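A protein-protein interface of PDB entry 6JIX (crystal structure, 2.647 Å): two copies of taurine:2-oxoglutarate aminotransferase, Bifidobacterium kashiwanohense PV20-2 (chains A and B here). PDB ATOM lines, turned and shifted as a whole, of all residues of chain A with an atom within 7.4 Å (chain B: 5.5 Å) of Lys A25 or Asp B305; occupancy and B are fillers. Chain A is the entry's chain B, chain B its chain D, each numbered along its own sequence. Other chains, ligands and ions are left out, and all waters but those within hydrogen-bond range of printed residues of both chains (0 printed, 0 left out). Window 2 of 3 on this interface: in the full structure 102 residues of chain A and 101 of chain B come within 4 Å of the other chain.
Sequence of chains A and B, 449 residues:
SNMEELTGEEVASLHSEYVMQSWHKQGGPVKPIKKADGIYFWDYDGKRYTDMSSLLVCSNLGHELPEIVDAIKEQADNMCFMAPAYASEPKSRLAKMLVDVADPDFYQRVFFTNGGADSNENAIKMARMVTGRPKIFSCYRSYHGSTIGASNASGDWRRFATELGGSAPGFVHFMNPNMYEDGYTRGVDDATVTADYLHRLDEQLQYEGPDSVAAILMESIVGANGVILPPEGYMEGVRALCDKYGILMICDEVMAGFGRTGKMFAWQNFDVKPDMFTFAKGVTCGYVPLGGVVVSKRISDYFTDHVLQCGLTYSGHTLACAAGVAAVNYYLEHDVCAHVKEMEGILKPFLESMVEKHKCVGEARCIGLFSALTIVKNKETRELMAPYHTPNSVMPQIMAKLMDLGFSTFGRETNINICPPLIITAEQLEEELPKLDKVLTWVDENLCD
O of Gln A21 touches CD2 of Leu B308 (3.4 Å).
Trp A23 touches Val B307.
His A24 touches Val B307 (O to CA, 3.8 Å).
Phe B303 touches Lys A25 (O to CA, 3.3 Å).
Thr B304 touches Lys A25 (O to CD, 3.5 Å).
CG of Lys A25 touches CG2 of Val B307, at 3.8 Å.
Thr B304 touches Gln A26 (CG2 to O, 3.7 Å).
NE2 of Gln A26 touches CB of Leu B308, 3.8 Å away.
The side-chain amino group (NZ) of Lys A25 is in hydrogen-bond range of the backbone carbonyl oxygen (O) of Asp B305 (2.9 Å).
O of His A24 sits at hydrogen-bond distance from N of Leu B308 (3.0 Å).
The backbone NH (N) of Gln A26 sits at hydrogen-bond distance from the backbone carbonyl oxygen (O) of Phe B303.
The backbone NH (N) of Trp A23 lies within hydrogen-bond range of the backbone carbonyl oxygen (O) of Leu B308.
The side-chain amide oxygen of Gln A26 sits at hydrogen-bond distance from the backbone NH of Gln A21 (2.6 Å).
The backbone carbonyl oxygen (O) of His A24 sits at hydrogen-bond distance from the side-chain amide nitrogen (NE2) of Gln A26.
OG1 of Thr B304 sits close to O of Asp B301, 3.3 Å away.
Of the 8 printed residues of chain B, 5 touch a printed residue of chain A.
Hydrophobic or aromatic side chains of chain B that line the printed part of chain A: Val B307 and Leu B308.
Among the printed residues, 12 pairs touch across the chains.
No position is printed for both chains.
Of the 12 pairs that touch across the chains among the printed residues, none has its exchanged pair printed and touching as well.
Of chain A, only Lys A25 comes within 4 Å of Asp B305.
Of the printed residues of chain A, Phe B303 touches Lys A25 (3.3 Å) and Gln A26 (2.7 Å).
Printed residues of chain B within 4 Å of Gln A26: Phe B303, Thr B304 and Leu B308.
Printed residues of chain A within 4 Å of Thr B304: Lys A25 (3.5 Å) and Gln A26 (3.7 Å).
Printed residues of chain B within 4 Å of Gln A21: Leu B308.
Of the printed residues of chain B, Trp A23 touches Val B307 (3.9 Å) and Leu B308 (3.1 Å).
Asp B301 touches none of the printed residues of chain A.
Gly A27 touches none of the printed residues of chain B.
The nearest printed residue of chain B that does not touch Gln A26 is His B306 (5.0 Å).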
ATOM      1  N   GLN A  21       8.770   1.339 -14.139  1.00  0.00           N
ATOM      2  CA  GLN A  21      10.015   0.593 -14.269  1.00  0.00           C
ATOM      3  C   GLN A  21      11.003   1.310 -15.190  1.00  0.00           C
ATOM      4  O   GLN A  21      10.638   1.758 -16.281  1.00  0.00           O
ATOM      5  CB  GLN A  21       9.708  -0.784 -14.837  1.00  0.00           C
ATOM      6  CG  GLN A  21      10.864  -1.704 -14.841  1.00  0.00           C
ATOM      7  CD  GLN A  21      11.354  -1.944 -13.465  1.00  0.00           C
ATOM      8  OE1 GLN A  21      10.852  -2.829 -12.762  1.00  0.00           O
ATOM      9  NE2 GLN A  21      12.335  -1.151 -13.043  1.00  0.00           N
ATOM     10  N   SER A  22      12.257   1.401 -14.762  1.00  0.00           N
ATOM     11  CA  SER A  22      13.288   1.990 -15.607  1.00  0.00           C
ATOM     12  C   SER A  22      13.607   1.100 -16.805  1.00  0.00           C
ATOM     13  O   SER A  22      13.691  -0.130 -16.683  1.00  0.00           O
ATOM     14  CB  SER A  22      14.563   2.237 -14.805  1.00  0.00           C
ATOM     15  OG  SER A  22      14.314   3.086 -13.703  1.00  0.00           O
ATOM     16  N   TRP A  23      13.773   1.745 -17.970  1.00  0.00           N
ATOM     17  CA  TRP A  23      14.338   1.142 -19.184  1.00  0.00           C
ATOM     18  C   TRP A  23      13.537  -0.058 -19.689  1.00  0.00           C
ATOM     19  O   TRP A  23      14.112  -0.999 -20.245  1.00  0.00           O
ATOM     20  CB  TRP A  23      15.800   0.735 -18.988  1.00  0.00           C
ATOM     21  CG  TRP A  23      16.704   1.756 -18.332  1.00  0.00           C
ATOM     22  CD1 TRP A  23      17.312   1.630 -17.125  1.00  0.00           C
ATOM     23  CD2 TRP A  23      17.139   3.023 -18.860  1.00  0.00           C
ATOM     24  NE1 TRP A  23      18.088   2.731 -16.848  1.00  0.00           N
ATOM     25  CE2 TRP A  23      18.000   3.605 -17.897  1.00  0.00           C
ATOM     26  CE3 TRP A  23      16.886   3.724 -20.047  1.00  0.00           C
ATOM     27  CZ2 TRP A  23      18.605   4.851 -18.081  1.00  0.00           C
ATOM     28  CZ3 TRP A  23      17.489   4.970 -20.228  1.00  0.00           C
ATOM     29  CH2 TRP A  23      18.339   5.516 -19.247  1.00  0.00           C
ATOM     30  N   HIS A  24      12.213  -0.031 -19.538  1.00  0.00           N
ATOM     31  CA  HIS A  24      11.362  -1.165 -19.896  1.00  0.00           C
ATOM     32  C   HIS A  24       9.994  -0.634 -20.306  1.00  0.00           C
ATOM     33  O   HIS A  24       9.650   0.517 -20.025  1.00  0.00           O
ATOM     34  CB  HIS A  24      11.220  -2.172 -18.738  1.00  0.00           C
ATOM     35  CG  HIS A  24      12.227  -3.286 -18.772  1.00  0.00           C
ATOM     36  ND1 HIS A  24      13.588  -3.071 -18.663  1.00  0.00           N
ATOM     37  CD2 HIS A  24      12.071  -4.628 -18.900  1.00  0.00           C
ATOM     38  CE1 HIS A  24      14.226  -4.228 -18.733  1.00  0.00           C
ATOM     39  NE2 HIS A  24      13.328  -5.188 -18.874  1.00  0.00           N
ATOM     40  N   LYS A  25       9.225  -1.466 -21.007  1.00  0.00           N
ATOM     41  CA  LYS A  25       7.808  -1.164 -21.136  1.00  0.00           C
ATOM     42  C   LYS A  25       7.125  -1.481 -19.814  1.00  0.00           C
ATOM     43  O   LYS A  25       7.537  -2.379 -19.083  1.00  0.00           O
ATOM     44  CB  LYS A  25       7.162  -1.959 -22.269  1.00  0.00           C
ATOM     45  CG  LYS A  25       8.003  -2.069 -23.510  1.00  0.00           C
ATOM     46  CD  LYS A  25       7.122  -2.251 -24.726  1.00  0.00           C
ATOM     47  CE  LYS A  25       7.929  -2.699 -25.943  1.00  0.00           C
ATOM     48  NZ  LYS A  25       7.349  -2.145 -27.213  1.00  0.00           N
ATOM     49  N   GLN A  26       6.055  -0.760 -19.525  1.00  0.00           N
ATOM     50  CA  GLN A  26       5.438  -0.896 -18.224  1.00  0.00           C
ATOM     51  C   GLN A  26       4.609  -2.171 -18.167  1.00  0.00           C
ATOM     52  O   GLN A  26       4.185  -2.710 -19.194  1.00  0.00           O
ATOM     53  CB  GLN A  26       4.552   0.317 -17.926  1.00  0.00           C
ATOM     54  CG  GLN A  26       5.311   1.577 -17.504  1.00  0.00           C
ATOM     55  CD  GLN A  26       6.704   1.287 -16.950  1.00  0.00           C
ATOM     56  OE1 GLN A  26       6.853   0.907 -15.790  1.00  0.00           O
ATOM     57  NE2 GLN A  26       7.729   1.463 -17.781  1.00  0.00           N
ATOM     58  N   GLY A  27       4.442  -2.693 -16.952  1.00  0.00           N
ATOM     59  CA  GLY A  27       3.449  -3.719 -16.701  1.00  0.00           C
ATOM     60  C   GLY A  27       3.856  -5.149 -16.981  1.00  0.00           C
ATOM     61  O   GLY A  27       2.991  -6.032 -16.937  1.00  0.00           O
ATOM     62  N   GLY A  28       5.134  -5.426 -17.247  1.00  0.00           N
ATOM     63  CA  GLY A  28       5.540  -6.785 -17.473  1.00  0.00           C
ATOM     64  C   GLY A  28       5.392  -7.646 -16.222  1.00  0.00           C
ATOM     65  O   GLY A  28       4.935  -7.184 -15.165  1.00  0.00           O
ATOM     66  N   PRO A  29       5.769  -8.917 -16.333  1.00  0.00           N
ATOM     67  CA  PRO A  29       5.951  -9.732 -15.126  1.00  0.00           C
ATOM     68  C   PRO A  29       7.205  -9.293 -14.374  1.00  0.00           C
ATOM     69  O   PRO A  29       8.135  -8.720 -14.953  1.00  0.00           O
ATOM     70  CB  PRO A  29       6.084 -11.153 -15.683  1.00  0.00           C
ATOM     71  CG  PRO A  29       6.674 -10.956 -17.046  1.00  0.00           C
ATOM     72  CD  PRO A  29       6.178  -9.630 -17.559  1.00  0.00           C
ATOM     73  N   ASP B 301      -0.284   4.350 -20.156  1.00  0.00           N
ATOM     74  CA  ASP B 301      -0.539   3.539 -21.340  1.00  0.00           C
ATOM     75  C   ASP B 301       0.544   3.726 -22.387  1.00  0.00           C
ATOM     76  O   ASP B 301       1.016   2.748 -22.973  1.00  0.00           O
ATOM     77  CB  ASP B 301      -1.903   3.877 -21.919  1.00  0.00           C
ATOM     78  CG  ASP B 301      -3.030   3.419 -21.036  1.00  0.00           C
ATOM     79  OD1 ASP B 301      -2.817   2.490 -20.220  1.00  0.00           O
ATOM     80  OD2 ASP B 301      -4.126   3.995 -21.160  1.00  0.00           O
ATOM     81  N   TYR B 302       0.953   4.973 -22.638  1.00  0.00           N
ATOM     82  CA  TYR B 302       1.959   5.210 -23.667  1.00  0.00           C
ATOM     83  C   TYR B 302       3.207   4.364 -23.435  1.00  0.00           C
ATOM     84  O   TYR B 302       3.744   3.771 -24.380  1.00  0.00           O
ATOM     85  CB  TYR B 302       2.329   6.700 -23.747  1.00  0.00           C
ATOM     86  CG  TYR B 302       3.413   6.958 -24.774  1.00  0.00           C
ATOM     87  CD1 TYR B 302       3.098   7.199 -26.102  1.00  0.00           C
ATOM     88  CD2 TYR B 302       4.758   6.900 -24.421  1.00  0.00           C
ATOM     89  CE1 TYR B 302       4.085   7.398 -27.038  1.00  0.00           C
ATOM     90  CE2 TYR B 302       5.756   7.093 -25.357  1.00  0.00           C
ATOM     91  CZ  TYR B 302       5.415   7.342 -26.665  1.00  0.00           C
ATOM     92  OH  TYR B 302       6.416   7.531 -27.599  1.00  0.00           O
ATOM     93  N   PHE B 303       3.682   4.287 -22.187  1.00  0.00           N
ATOM     94  CA  PHE B 303       4.896   3.545 -21.851  1.00  0.00           C
ATOM     95  C   PHE B 303       4.642   2.061 -21.606  1.00  0.00           C
ATOM     96  O   PHE B 303       5.573   1.329 -21.236  1.00  0.00           O
ATOM     97  CB  PHE B 303       5.573   4.180 -20.641  1.00  0.00           C
ATOM     98  CG  PHE B 303       6.248   5.479 -20.959  1.00  0.00           C
ATOM     99  CD1 PHE B 303       7.379   5.507 -21.750  1.00  0.00           C
ATOM    100  CD2 PHE B 303       5.749   6.665 -20.488  1.00  0.00           C
ATOM    101  CE1 PHE B 303       8.003   6.688 -22.045  1.00  0.00           C
ATOM    102  CE2 PHE B 303       6.367   7.848 -20.791  1.00  0.00           C
ATOM    103  CZ  PHE B 303       7.494   7.853 -21.570  1.00  0.00           C
ATOM    104  N   THR B 304       3.404   1.611 -21.797  1.00  0.00           N
ATOM    105  CA  THR B 304       3.132   0.191 -21.972  1.00  0.00           C
ATOM    106  C   THR B 304       3.450  -0.256 -23.393  1.00  0.00           C
ATOM    107  O   THR B 304       3.901  -1.384 -23.612  1.00  0.00           O
ATOM    108  CB  THR B 304       1.672  -0.102 -21.640  1.00  0.00           C
ATOM    109  OG1 THR B 304       1.299   0.617 -20.457  1.00  0.00           O
ATOM    110  CG2 THR B 304       1.485  -1.575 -21.424  1.00  0.00           C
ATOM    111  N   ASP B 305       3.205   0.613 -24.368  1.00  0.00           N
ATOM    112  CA  ASP B 305       3.530   0.321 -25.757  1.00  0.00           C
ATOM    113  C   ASP B 305       4.956   0.696 -26.122  1.00  0.00           C
ATOM    114  O   ASP B 305       5.537   0.066 -27.015  1.00  0.00           O
ATOM    115  CB  ASP B 305       2.558   1.053 -26.684  1.00  0.00           C
ATOM    116  CG  ASP B 305       1.148   0.537 -26.548  1.00  0.00           C
ATOM    117  OD1 ASP B 305       0.982  -0.698 -26.441  1.00  0.00           O
ATOM    118  OD2 ASP B 305       0.206   1.351 -26.530  1.00  0.00           O
ATOM    119  N   HIS B 306       5.542   1.683 -25.435  1.00  0.00           N
ATOM    120  CA  HIS B 306       6.885   2.167 -25.730  1.00  0.00           C
ATOM    121  C   HIS B 306       7.773   2.032 -24.501  1.00  0.00           C
ATOM    122  O   HIS B 306       7.329   2.226 -23.366  1.00  0.00           O
ATOM    123  CB  HIS B 306       6.887   3.636 -26.168  1.00  0.00           C
ATOM    124  CG  HIS B 306       5.934   3.937 -27.284  1.00  0.00           C
ATOM    125  ND1 HIS B 306       4.581   4.117 -27.082  1.00  0.00           N
ATOM    126  CD2 HIS B 306       6.142   4.087 -28.615  1.00  0.00           C
ATOM    127  CE1 HIS B 306       3.997   4.363 -28.242  1.00  0.00           C
ATOM    128  NE2 HIS B 306       4.922   4.349 -29.188  1.00  0.00           N
ATOM    129  N   VAL B 307       9.050   1.737 -24.746  1.00  0.00           N
ATOM    130  CA  VAL B 307      10.016   1.613 -23.668  1.00  0.00           C
ATOM    131  C   VAL B 307      10.207   2.973 -23.019  1.00  0.00           C
ATOM    132  O   VAL B 307      10.440   3.978 -23.705  1.00  0.00           O
ATOM    133  CB  VAL B 307      11.345   1.061 -24.202  1.00  0.00           C
ATOM    134  CG1 VAL B 307      12.428   1.199 -23.156  1.00  0.00           C
ATOM    135  CG2 VAL B 307      11.179  -0.385 -24.647  1.00  0.00           C
ATOM    136  N   LEU B 308      10.089   3.017 -21.695  1.00  0.00           N
ATOM    137  CA  LEU B 308      10.402   4.210 -20.912  1.00  0.00           C
ATOM    138  C   LEU B 308      11.913   4.364 -20.843  1.00  0.00           C
ATOM    139  O   LEU B 308      12.586   3.649 -20.095  1.00  0.00           O
ATOM    140  CB  LEU B 308       9.794   4.106 -19.520  1.00  0.00           C
ATOM    141  CG  LEU B 308      10.233   5.162 -18.511  1.00  0.00           C
ATOM    142  CD1 LEU B 308       9.835   6.571 -18.977  1.00  0.00           C
ATOM    143  CD2 LEU B 308       9.656   4.855 -17.128  1.00  0.00           C
